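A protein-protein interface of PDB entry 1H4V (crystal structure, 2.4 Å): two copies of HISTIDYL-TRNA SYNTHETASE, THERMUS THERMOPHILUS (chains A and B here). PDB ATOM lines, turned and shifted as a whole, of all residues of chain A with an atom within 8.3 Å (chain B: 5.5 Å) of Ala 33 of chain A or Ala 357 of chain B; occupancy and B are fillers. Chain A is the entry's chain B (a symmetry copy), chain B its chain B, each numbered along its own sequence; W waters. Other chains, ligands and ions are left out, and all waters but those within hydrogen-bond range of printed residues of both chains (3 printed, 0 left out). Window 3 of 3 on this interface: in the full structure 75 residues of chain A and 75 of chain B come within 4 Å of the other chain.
N of Ala 357 of chain B lies within hydrogen-bond range of O of Ala 33 of chain A.
The side-chain carboxylate of Glu 142 of chain A is in salt-bridge range of the guanidinium group of Arg 352 of chain B, 3.0 Å away.
The side-chain carboxylate (OE1) of Glu 142 of chain A sits at hydrogen-bond distance from the side-chain hydroxyl (OH) of Tyr 359 of chain B (2.9 Å).
OH of Tyr 359 of chain B lies within hydrogen-bond range of NH2 of Arg 103 of chain A (3.3 Å).
The backbone carbonyl oxygen (O) of Glu 32 of chain A sits close to the guanidinium group (NE) of Arg 356 of chain B (3.5 Å).
NE1 of Trp 105 of chain A is in hydrogen-bond range of OE2 of Glu 32 of chain A, 3.2 Å away.
OE2 of Glu 142 of chain A lies within salt-bridge range of NE of Arg 103 of chain A, 2.8 Å away.
O of Leu 331 of chain B sits at hydrogen-bond distance from N of Glu 358 of chain B (2.7 Å).
The side-chain carboxylate (OE2) of Glu 358 of chain B lies within salt-bridge range of the guanidinium group (NE) of Arg 356 of chain B (3.0 Å).
N of Leu 331 of chain B lies within hydrogen-bond range of O of Arg 356 of chain B (3.1 Å).
The backbone carbonyl oxygen (O) of Ala 357 of chain B lies within hydrogen-bond range of the guanidinium group (NH2) of Arg 352 of chain B.
CB of Pro 353 of chain B touches CA of Val 30 of chain A, 3.9 Å away.
Arg 352 of chain B touches Ala 33 of chain A (NE to O, 3.8 Å).
Pro 353 of chain B touches Ala 33 of chain A (O to CB, 3.99 Å).
CB of Ala 33 of chain A touches O of Leu 355 of chain B, at 3.9 Å.
CG of Arg 356 of chain B touches O of Ala 33 of chain A, 3.5 Å away.
CZ of Arg 352 of chain B touches CB of Ala 34 of chain A, 3.5 Å away.
Glu 358 of chain B touches Gly 35 of chain A (CD to CA, 3.7 Å).
Of the printed residues of chain B, Ala 33 of chain A touches Arg 352, Pro 353, Leu 355, Arg 356 and Ala 357.
Of the printed residues of chain A, Ala 357 of chain B touches Ala 33 (3.3 Å).
Printed residues of chain A within 4 Å of Arg 352 of chain B: Ala 33 (3.8 Å), Ala 34 (3.5 Å) and Glu 142 (3.0 Å).
Of the printed residues of chain A, Leu 355 of chain B touches Ala 33.
Printed residues of chain B within 4 Å of Gly 35 of chain A: Glu 358 (3.7 Å).
Printed residues of chain A within 4 Å of Glu 358 of chain B: Gly 35 (3.7 Å).
The nearest residue of chain A that does not touch Ala 357 of chain B is Ala 34 of chain A (4.6 Å).
The nearest printed residue of chain A that does not touch Leu 355 of chain B is Ala 34 of chain A (6.1 Å).
Hydrophobic or aromatic side chains of chain A within 4 Å of the printed part of chain B: Ala 33 and Ala 34.
Of the 14 printed residues of chain B, 7 touch a printed residue of chain A.
Printed residues of chain B that touch a printed residue of chain A: Arg 352, Pro 353, Leu 355, Arg 356, Ala 357, Glu 358 and Tyr 359.
Hydrophobic or aromatic side chains of chain B that line the printed part of chain A: Pro 353 and Tyr 359.
Along chain B the printed residues that touch a printed residue of chain A span positions 352 to 359.
Among the printed residues, Asp or Glu carboxylates within 4 Å of a Lys or Arg side-chain nitrogen of the other chain: Glu 142 of chain A with Arg 352 of chain B (3.0 Å).
No position is printed for both chains.
Water W2 lies within hydrogen-bond range of NH2 of Arg 352 of chain B (2.6 Å), O of Ala 34 of chain A (2.7 Å), OE1 of Glu 142 of chain A (2.8 Å) and NE of Arg 103 of chain A (3.2 Å).
Water W1 lies within hydrogen-bond range of the guanidinium group of Arg 103 of chain A (2.7 Å) and the backbone carbonyl oxygen of Tyr 359 of chain B (2.8 Å).
Water W3 lies within hydrogen-bond range of the backbone carbonyl oxygen (O) of Glu 32 of chain A (2.8 Å), the backbone carbonyl oxygen (O) of Ala 36 of chain A (3.1 Å) and the guanidinium group (NH2) of Arg 356 of chain B (3.5 Å).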
ATOM      1  N   THR A  26      -6.661  -9.980  24.572  1.00  0.00           N
ATOM      2  CA  THR A  26      -6.887  -8.713  23.902  1.00  0.00           C
ATOM      3  C   THR A  26      -8.361  -8.313  23.969  1.00  0.00           C
ATOM      4  O   THR A  26      -8.683  -7.160  24.247  1.00  0.00           O
ATOM      5  CB  THR A  26      -6.445  -8.781  22.448  1.00  0.00           C
ATOM      6  OG1 THR A  26      -5.022  -8.935  22.407  1.00  0.00           O
ATOM      7  CG2 THR A  26      -6.845  -7.516  21.705  1.00  0.00           C
ATOM      8  N   ALA A  27      -9.259  -9.263  23.719  1.00  0.00           N
ATOM      9  CA  ALA A  27     -10.686  -8.965  23.788  1.00  0.00           C
ATOM     10  C   ALA A  27     -11.007  -8.539  25.222  1.00  0.00           C
ATOM     11  O   ALA A  27     -11.751  -7.581  25.441  1.00  0.00           O
ATOM     12  CB  ALA A  27     -11.515 -10.195  23.408  1.00  0.00           C
ATOM     13  N   ARG A  28     -10.438  -9.241  26.198  1.00  0.00           N
ATOM     14  CA  ARG A  28     -10.702  -8.899  27.584  1.00  0.00           C
ATOM     15  C   ARG A  28     -10.310  -7.448  27.872  1.00  0.00           C
ATOM     16  O   ARG A  28     -11.063  -6.721  28.525  1.00  0.00           O
ATOM     17  CB  ARG A  28      -9.964  -9.842  28.551  1.00  0.00           C
ATOM     18  CG  ARG A  28     -10.035  -9.381  30.008  1.00  0.00           C
ATOM     19  CD  ARG A  28      -9.340 -10.317  30.994  1.00  0.00           C
ATOM     20  NE  ARG A  28     -10.121 -11.523  31.270  1.00  0.00           N
ATOM     21  CZ  ARG A  28      -9.846 -12.733  30.785  1.00  0.00           C
ATOM     22  NH1 ARG A  28      -8.793 -12.914  29.990  1.00  0.00           N
ATOM     23  NH2 ARG A  28     -10.630 -13.761  31.082  1.00  0.00           N
ATOM     24  N   LYS A  29      -9.150  -7.024  27.375  1.00  0.00           N
ATOM     25  CA  LYS A  29      -8.686  -5.655  27.606  1.00  0.00           C
ATOM     26  C   LYS A  29      -9.605  -4.606  26.985  1.00  0.00           C
ATOM     27  O   LYS A  29      -9.997  -3.649  27.652  1.00  0.00           O
ATOM     28  CB  LYS A  29      -7.261  -5.457  27.062  1.00  0.00           C
ATOM     29  CG  LYS A  29      -6.736  -4.020  27.204  1.00  0.00           C
ATOM     30  CD  LYS A  29      -5.330  -3.856  26.632  1.00  0.00           C
ATOM     31  CE  LYS A  29      -5.314  -3.938  25.100  1.00  0.00           C
ATOM     32  NZ  LYS A  29      -3.973  -3.620  24.509  1.00  0.00           N
ATOM     33  N   VAL A  30      -9.956  -4.776  25.714  1.00  0.00           N
ATOM     34  CA  VAL A  30     -10.816  -3.790  25.067  1.00  0.00           C
ATOM     35  C   VAL A  30     -12.258  -3.821  25.574  1.00  0.00           C
ATOM     36  O   VAL A  30     -12.860  -2.774  25.791  1.00  0.00           O
ATOM     37  CB  VAL A  30     -10.814  -3.943  23.508  1.00  0.00           C
ATOM     38  CG1 VAL A  30      -9.408  -4.230  23.009  1.00  0.00           C
ATOM     39  CG2 VAL A  30     -11.762  -5.014  23.083  1.00  0.00           C
ATOM     40  N   LEU A  31     -12.807  -5.013  25.778  1.00  0.00           N
ATOM     41  CA  LEU A  31     -14.183  -5.123  26.249  1.00  0.00           C
ATOM     42  C   LEU A  31     -14.368  -4.671  27.696  1.00  0.00           C
ATOM     43  O   LEU A  31     -15.392  -4.071  28.027  1.00  0.00           O
ATOM     44  CB  LEU A  31     -14.688  -6.560  26.064  1.00  0.00           C
ATOM     45  CG  LEU A  31     -15.427  -6.904  24.759  1.00  0.00           C
ATOM     46  CD1 LEU A  31     -15.028  -5.989  23.634  1.00  0.00           C
ATOM     47  CD2 LEU A  31     -15.166  -8.367  24.393  1.00  0.00           C
ATOM     48  N   GLU A  32     -13.394  -4.931  28.563  1.00  0.00           N
ATOM     49  CA  GLU A  32     -13.552  -4.511  29.952  1.00  0.00           C
ATOM     50  C   GLU A  32     -13.252  -3.019  30.137  1.00  0.00           C
ATOM     51  O   GLU A  32     -13.647  -2.422  31.137  1.00  0.00           O
ATOM     52  CB  GLU A  32     -12.713  -5.392  30.897  1.00  0.00           C
ATOM     53  CG  GLU A  32     -13.210  -6.857  30.887  1.00  0.00           C
ATOM     54  CD  GLU A  32     -12.656  -7.727  32.000  1.00  0.00           C
ATOM     55  OE1 GLU A  32     -11.486  -7.538  32.402  1.00  0.00           O
ATOM     56  OE2 GLU A  32     -13.390  -8.625  32.466  1.00  0.00           O
ATOM     57  N   ALA A  33     -12.585  -2.416  29.154  1.00  0.00           N
ATOM     58  CA  ALA A  33     -12.289  -0.989  29.211  1.00  0.00           C
ATOM     59  C   ALA A  33     -13.568  -0.256  28.834  1.00  0.00           C
ATOM     60  O   ALA A  33     -13.738   0.918  29.163  1.00  0.00           O
ATOM     61  CB  ALA A  33     -11.185  -0.628  28.237  1.00  0.00           C
ATOM     62  N   ALA A  34     -14.466  -0.947  28.132  1.00  0.00           N
ATOM     63  CA  ALA A  34     -15.731  -0.339  27.734  1.00  0.00           C
ATOM     64  C   ALA A  34     -16.844  -0.704  28.705  1.00  0.00           C
ATOM     65  O   ALA A  34     -18.022  -0.512  28.421  1.00  0.00           O
ATOM     66  CB  ALA A  34     -16.097  -0.754  26.344  1.00  0.00           C
ATOM     67  N   GLY A  35     -16.463  -1.235  29.861  1.00  0.00           N
ATOM     68  CA  GLY A  35     -17.448  -1.584  30.866  1.00  0.00           C
ATOM     69  C   GLY A  35     -18.046  -2.978  30.848  1.00  0.00           C
ATOM     70  O   GLY A  35     -18.816  -3.305  31.740  1.00  0.00           O
ATOM     71  N   ALA A  36     -17.713  -3.809  29.870  1.00  0.00           N
ATOM     72  CA  ALA A  36     -18.293  -5.151  29.839  1.00  0.00           C
ATOM     73  C   ALA A  36     -17.849  -5.981  31.042  1.00  0.00           C
ATOM     74  O   ALA A  36     -16.706  -5.910  31.469  1.00  0.00           O
ATOM     75  CB  ALA A  36     -17.919  -5.847  28.560  1.00  0.00           C
ATOM     76  N   LEU A  37     -18.778  -6.751  31.592  1.00  0.00           N
ATOM     77  CA  LEU A  37     -18.520  -7.618  32.744  1.00  0.00           C
ATOM     78  C   LEU A  37     -18.304  -9.045  32.219  1.00  0.00           C
ATOM     79  O   LEU A  37     -19.054  -9.504  31.357  1.00  0.00           O
ATOM     80  CB  LEU A  37     -19.734  -7.570  33.668  1.00  0.00           C
ATOM     81  CG  LEU A  37     -19.784  -8.379  34.961  1.00  0.00           C
ATOM     82  CD1 LEU A  37     -18.647  -7.964  35.893  1.00  0.00           C
ATOM     83  CD2 LEU A  37     -21.137  -8.128  35.629  1.00  0.00           C
ATOM     84  N   ARG A 103     -23.573  -4.555  30.039  1.00  0.00           N
ATOM     85  CA  ARG A 103     -22.643  -5.016  29.030  1.00  0.00           C
ATOM     86  C   ARG A 103     -21.951  -6.279  29.525  1.00  0.00           C
ATOM     87  O   ARG A 103     -21.390  -6.313  30.620  1.00  0.00           O
ATOM     88  CB  ARG A 103     -21.621  -3.916  28.710  1.00  0.00           C
ATOM     89  CG  ARG A 103     -22.216  -2.681  28.021  1.00  0.00           C
ATOM     90  CD  ARG A 103     -21.104  -1.710  27.618  1.00  0.00           C
ATOM     91  NE  ARG A 103     -21.589  -0.486  26.982  1.00  0.00           N
ATOM     92  CZ  ARG A 103     -22.210   0.501  27.622  1.00  0.00           C
ATOM     93  NH1 ARG A 103     -22.439   0.425  28.929  1.00  0.00           N
ATOM     94  NH2 ARG A 103     -22.578   1.582  26.957  1.00  0.00           N
ATOM     95  N   TRP A 105     -19.486  -9.911  28.379  1.00  0.00           N
ATOM     96  CA  TRP A 105     -18.635 -10.527  27.386  1.00  0.00           C
ATOM     97  C   TRP A 105     -18.264 -11.896  27.910  1.00  0.00           C
ATOM     98  O   TRP A 105     -18.326 -12.159  29.117  1.00  0.00           O
ATOM     99  CB  TRP A 105     -17.383  -9.690  27.084  1.00  0.00           C
ATOM    100  CG  TRP A 105     -16.281  -9.816  28.079  1.00  0.00           C
ATOM    101  CD1 TRP A 105     -16.127  -9.105  29.234  1.00  0.00           C
ATOM    102  CD2 TRP A 105     -15.166 -10.705  28.000  1.00  0.00           C
ATOM    103  NE1 TRP A 105     -14.979  -9.494  29.880  1.00  0.00           N
ATOM    104  CE2 TRP A 105     -14.370 -10.479  29.149  1.00  0.00           C
ATOM    105  CE3 TRP A 105     -14.763 -11.678  27.075  1.00  0.00           C
ATOM    106  CZ2 TRP A 105     -13.183 -11.186  29.396  1.00  0.00           C
ATOM    107  CZ3 TRP A 105     -13.578 -12.383  27.322  1.00  0.00           C
ATOM    108  CH2 TRP A 105     -12.806 -12.131  28.478  1.00  0.00           C
ATOM    109  N   GLU A 142     -21.310   1.219  19.074  1.00  0.00           N
ATOM    110  CA  GLU A 142     -20.288   0.774  20.016  1.00  0.00           C
ATOM    111  C   GLU A 142     -19.939  -0.694  19.785  1.00  0.00           C
ATOM    112  O   GLU A 142     -18.766  -1.064  19.807  1.00  0.00           O
ATOM    113  CB  GLU A 142     -20.764   0.987  21.455  1.00  0.00           C
ATOM    114  CG  GLU A 142     -19.777   0.561  22.513  1.00  0.00           C
ATOM    115  CD  GLU A 142     -20.168   1.046  23.904  1.00  0.00           C
ATOM    116  OE1 GLU A 142     -19.417   1.854  24.497  1.00  0.00           O
ATOM    117  OE2 GLU A 142     -21.231   0.622  24.405  1.00  0.00           O
ATOM    118  N   LEU A 146     -16.284  -1.733  18.881  1.00  0.00           N
ATOM    119  CA  LEU A 146     -15.619  -2.645  19.810  1.00  0.00           C
ATOM    120  C   LEU A 146     -15.059  -3.880  19.093  1.00  0.00           C
ATOM    121  O   LEU A 146     -13.947  -4.315  19.387  1.00  0.00           O
ATOM    122  CB  LEU A 146     -16.575  -3.089  20.920  1.00  0.00           C
ATOM    123  CG  LEU A 146     -16.809  -2.127  22.089  1.00  0.00           C
ATOM    124  CD1 LEU A 146     -17.729  -2.782  23.094  1.00  0.00           C
ATOM    125  CD2 LEU A 146     -15.489  -1.766  22.755  1.00  0.00           C
ATOM    126  N   PRO B 329     -13.812   2.225  36.680  1.00  0.00           N
ATOM    127  CA  PRO B 329     -13.190   2.791  35.485  1.00  0.00           C
ATOM    128  C   PRO B 329     -12.295   3.968  35.846  1.00  0.00           C
ATOM    129  O   PRO B 329     -12.440   4.561  36.917  1.00  0.00           O
ATOM    130  CB  PRO B 329     -14.391   3.224  34.656  1.00  0.00           C
ATOM    131  CG  PRO B 329     -15.349   3.655  35.707  1.00  0.00           C
ATOM    132  CD  PRO B 329     -15.251   2.526  36.704  1.00  0.00           C
ATOM    133  N   ASP B 330     -11.370   4.299  34.953  1.00  0.00           N
ATOM    134  CA  ASP B 330     -10.484   5.432  35.182  1.00  0.00           C
ATOM    135  C   ASP B 330     -11.270   6.725  34.989  1.00  0.00           C
ATOM    136  O   ASP B 330     -10.971   7.735  35.615  1.00  0.00           O
ATOM    137  CB  ASP B 330      -9.300   5.402  34.212  1.00  0.00           C
ATOM    138  CG  ASP B 330      -8.400   4.201  34.428  1.00  0.00           C
ATOM    139  OD1 ASP B 330      -8.090   3.892  35.596  1.00  0.00           O
ATOM    140  OD2 ASP B 330      -7.996   3.568  33.434  1.00  0.00           O
ATOM    141  N   LEU B 331     -12.286   6.680  34.131  1.00  0.00           N
ATOM    142  CA  LEU B 331     -13.104   7.853  33.851  1.00  0.00           C
ATOM    143  C   LEU B 331     -14.573   7.509  33.596  1.00  0.00           C
ATOM    144  O   LEU B 331     -14.882   6.630  32.786  1.00  0.00           O
ATOM    145  CB  LEU B 331     -12.542   8.589  32.627  1.00  0.00           C
ATOM    146  CG  LEU B 331     -13.330   9.784  32.061  1.00  0.00           C
ATOM    147  CD1 LEU B 331     -13.268  10.946  33.045  1.00  0.00           C
ATOM    148  CD2 LEU B 331     -12.744  10.212  30.706  1.00  0.00           C
ATOM    149  N   TYR B 332     -15.472   8.198  34.296  1.00  0.00           N
ATOM    150  CA  TYR B 332     -16.905   8.011  34.108  1.00  0.00           C
ATOM    151  C   TYR B 332     -17.467   9.357  33.646  1.00  0.00           C
ATOM    152  O   TYR B 332     -17.567  10.306  34.426  1.00  0.00           O
ATOM    153  CB  TYR B 332     -17.596   7.583  35.401  1.00  0.00           C
ATOM    154  CG  TYR B 332     -19.019   7.132  35.170  1.00  0.00           C
ATOM    155  CD1 TYR B 332     -19.289   5.952  34.481  1.00  0.00           C
ATOM    156  CD2 TYR B 332     -20.094   7.912  35.579  1.00  0.00           C
ATOM    157  CE1 TYR B 332     -20.597   5.561  34.198  1.00  0.00           C
ATOM    158  CE2 TYR B 332     -21.407   7.532  35.301  1.00  0.00           C
ATOM    159  CZ  TYR B 332     -21.651   6.358  34.610  1.00  0.00           C
ATOM    160  OH  TYR B 332     -22.945   5.990  34.311  1.00  0.00           O
ATOM    161  N   LEU B 333     -17.819   9.426  32.366  1.00  0.00           N
ATOM    162  CA  LEU B 333     -18.345  10.636  31.735  1.00  0.00           C
ATOM    163  C   LEU B 333     -19.833  10.868  31.930  1.00  0.00           C
ATOM    164  O   LEU B 333     -20.652   9.988  31.674  1.00  0.00           O
ATOM    165  CB  LEU B 333     -18.048  10.601  30.239  1.00  0.00           C
ATOM    166  CG  LEU B 333     -16.628  11.004  29.864  1.00  0.00           C
ATOM    167  CD1 LEU B 333     -16.259  10.447  28.498  1.00  0.00           C
ATOM    168  CD2 LEU B 333     -16.531  12.525  29.893  1.00  0.00           C
ATOM    169  N   ALA B 348     -15.007   8.830  25.211  1.00  0.00           N
ATOM    170  CA  ALA B 348     -14.624   7.579  25.858  1.00  0.00           C
ATOM    171  C   ALA B 348     -13.934   6.649  24.843  1.00  0.00           C
ATOM    172  O   ALA B 348     -12.926   6.015  25.156  1.00  0.00           O
ATOM    173  CB  ALA B 348     -15.849   6.896  26.457  1.00  0.00           C
ATOM    174  N   LEU B 351     -10.375   7.395  24.304  1.00  0.00           N
ATOM    175  CA  LEU B 351      -9.515   7.083  25.437  1.00  0.00           C
ATOM    176  C   LEU B 351      -9.278   5.584  25.644  1.00  0.00           C
ATOM    177  O   LEU B 351      -8.368   5.195  26.374  1.00  0.00           O
ATOM    178  CB  LEU B 351     -10.114   7.706  26.707  1.00  0.00           C
ATOM    179  CG  LEU B 351     -10.186   9.242  26.687  1.00  0.00           C
ATOM    180  CD1 LEU B 351     -11.002   9.752  27.858  1.00  0.00           C
ATOM    181  CD2 LEU B 351      -8.764   9.817  26.723  1.00  0.00           C
ATOM    182  N   ARG B 352     -10.103   4.752  25.011  1.00  0.00           N
ATOM    183  CA  ARG B 352      -9.985   3.293  25.128  1.00  0.00           C
ATOM    184  C   ARG B 352      -9.061   2.747  24.048  1.00  0.00           C
ATOM    185  O   ARG B 352      -8.932   3.343  22.982  1.00  0.00           O
ATOM    186  CB  ARG B 352     -11.335   2.611  24.935  1.00  0.00           C
ATOM    187  CG  ARG B 352     -12.431   2.998  25.870  1.00  0.00           C
ATOM    188  CD  ARG B 352     -13.757   2.675  25.194  1.00  0.00           C
ATOM    189  NE  ARG B 352     -14.873   2.864  26.094  1.00  0.00           N
ATOM    190  CZ  ARG B 352     -16.144   2.696  25.759  1.00  0.00           C
ATOM    191  NH1 ARG B 352     -16.470   2.333  24.520  1.00  0.00           N
ATOM    192  NH2 ARG B 352     -17.084   2.877  26.678  1.00  0.00           N
ATOM    193  N   PRO B 353      -8.444   1.578  24.294  1.00  0.00           N
ATOM    194  CA  PRO B 353      -8.570   0.795  25.530  1.00  0.00           C
ATOM    195  C   PRO B 353      -7.453   1.046  26.546  1.00  0.00           C
ATOM    196  O   PRO B 353      -7.383   0.365  27.569  1.00  0.00           O
ATOM    197  CB  PRO B 353      -8.544  -0.632  25.015  1.00  0.00           C
ATOM    198  CG  PRO B 353      -7.524  -0.537  23.936  1.00  0.00           C
ATOM    199  CD  PRO B 353      -7.928   0.732  23.204  1.00  0.00           C
ATOM    200  N   LEU B 355      -7.174   3.372  28.532  1.00  0.00           N
ATOM    201  CA  LEU B 355      -7.805   3.806  29.766  1.00  0.00           C
ATOM    202  C   LEU B 355      -9.188   3.186  29.793  1.00  0.00           C
ATOM    203  O   LEU B 355      -9.765   2.937  28.743  1.00  0.00           O
ATOM    204  CB  LEU B 355      -7.925   5.332  29.770  1.00  0.00           C
ATOM    205  CG  LEU B 355      -7.165   6.201  30.772  1.00  0.00           C
ATOM    206  CD1 LEU B 355      -5.797   5.624  31.103  1.00  0.00           C
ATOM    207  CD2 LEU B 355      -7.033   7.589  30.172  1.00  0.00           C
ATOM    208  N   ARG B 356      -9.711   2.904  30.979  1.00  0.00           N
ATOM    209  CA  ARG B 356     -11.060   2.372  31.069  1.00  0.00           C
ATOM    210  C   ARG B 356     -11.977   3.591  31.231  1.00  0.00           C
ATOM    211  O   ARG B 356     -11.986   4.247  32.277  1.00  0.00           O
ATOM    212  CB  ARG B 356     -11.193   1.434  32.263  1.00  0.00           C
ATOM    213  CG  ARG B 356     -12.591   0.849  32.425  1.00  0.00           C
ATOM    214  CD  ARG B 356     -12.639  -0.193  33.532  1.00  0.00           C
ATOM    215  NE  ARG B 356     -14.003  -0.425  33.982  1.00  0.00           N
ATOM    216  CZ  ARG B 356     -14.321  -1.079  35.094  1.00  0.00           C
ATOM    217  NH1 ARG B 356     -13.368  -1.573  35.871  1.00  0.00           N
ATOM    218  NH2 ARG B 356     -15.596  -1.218  35.444  1.00  0.00           N
ATOM    219  N   ALA B 357     -12.734   3.907  30.188  1.00  0.00           N
ATOM    220  CA  ALA B 357     -13.621   5.066  30.229  1.00  0.00           C
ATOM    221  C   ALA B 357     -15.060   4.689  29.930  1.00  0.00           C
ATOM    222  O   ALA B 357     -15.354   4.098  28.892  1.00  0.00           O
ATOM    223  CB  ALA B 357     -13.138   6.122  29.238  1.00  0.00           C
ATOM    224  N   GLU B 358     -15.955   5.036  30.848  1.00  0.00           N
ATOM    225  CA  GLU B 358     -17.364   4.733  30.683  1.00  0.00           C
ATOM    226  C   GLU B 358     -18.193   6.005  30.670  1.00  0.00           C
ATOM    227  O   GLU B 358     -17.702   7.083  30.992  1.00  0.00           O
ATOM    228  CB  GLU B 358     -17.821   3.788  31.795  1.00  0.00           C
ATOM    229  CG  GLU B 358     -17.162   2.414  31.699  1.00  0.00           C
ATOM    230  CD  GLU B 358     -17.498   1.500  32.867  1.00  0.00           C
ATOM    231  OE1 GLU B 358     -18.702   1.272  33.118  1.00  0.00           O
ATOM    232  OE2 GLU B 358     -16.555   1.005  33.527  1.00  0.00           O
ATOM    233  N   TYR B 359     -19.458   5.880  30.301  1.00  0.00           N
ATOM    234  CA  TYR B 359     -20.318   7.045  30.219  1.00  0.00           C
ATOM    235  C   TYR B 359     -21.777   6.676  30.443  1.00  0.00           C
ATOM    236  O   TYR B 359     -22.181   5.544  30.197  1.00  0.00           O
ATOM    237  CB  TYR B 359     -20.156   7.676  28.835  1.00  0.00           C
ATOM    238  CG  TYR B 359     -20.498   6.715  27.718  1.00  0.00           C
ATOM    239  CD1 TYR B 359     -21.826   6.493  27.344  1.00  0.00           C
ATOM    240  CD2 TYR B 359     -19.505   5.962  27.092  1.00  0.00           C
ATOM    241  CE1 TYR B 359     -22.153   5.541  26.385  1.00  0.00           C
ATOM    242  CE2 TYR B 359     -19.824   5.008  26.130  1.00  0.00           C
ATOM    243  CZ  TYR B 359     -21.150   4.802  25.786  1.00  0.00           C
ATOM    244  OH  TYR B 359     -21.476   3.825  24.876  1.00  0.00           O
HETATM  245  O   HOH W   1     -23.335   3.385  28.824  1.00  0.00           O
HETATM  246  O   HOH W   2     -19.230   1.625  27.260  1.00  0.00           O
HETATM  247  O   HOH W   3     -15.206  -3.711  33.070  1.00  0.00           O
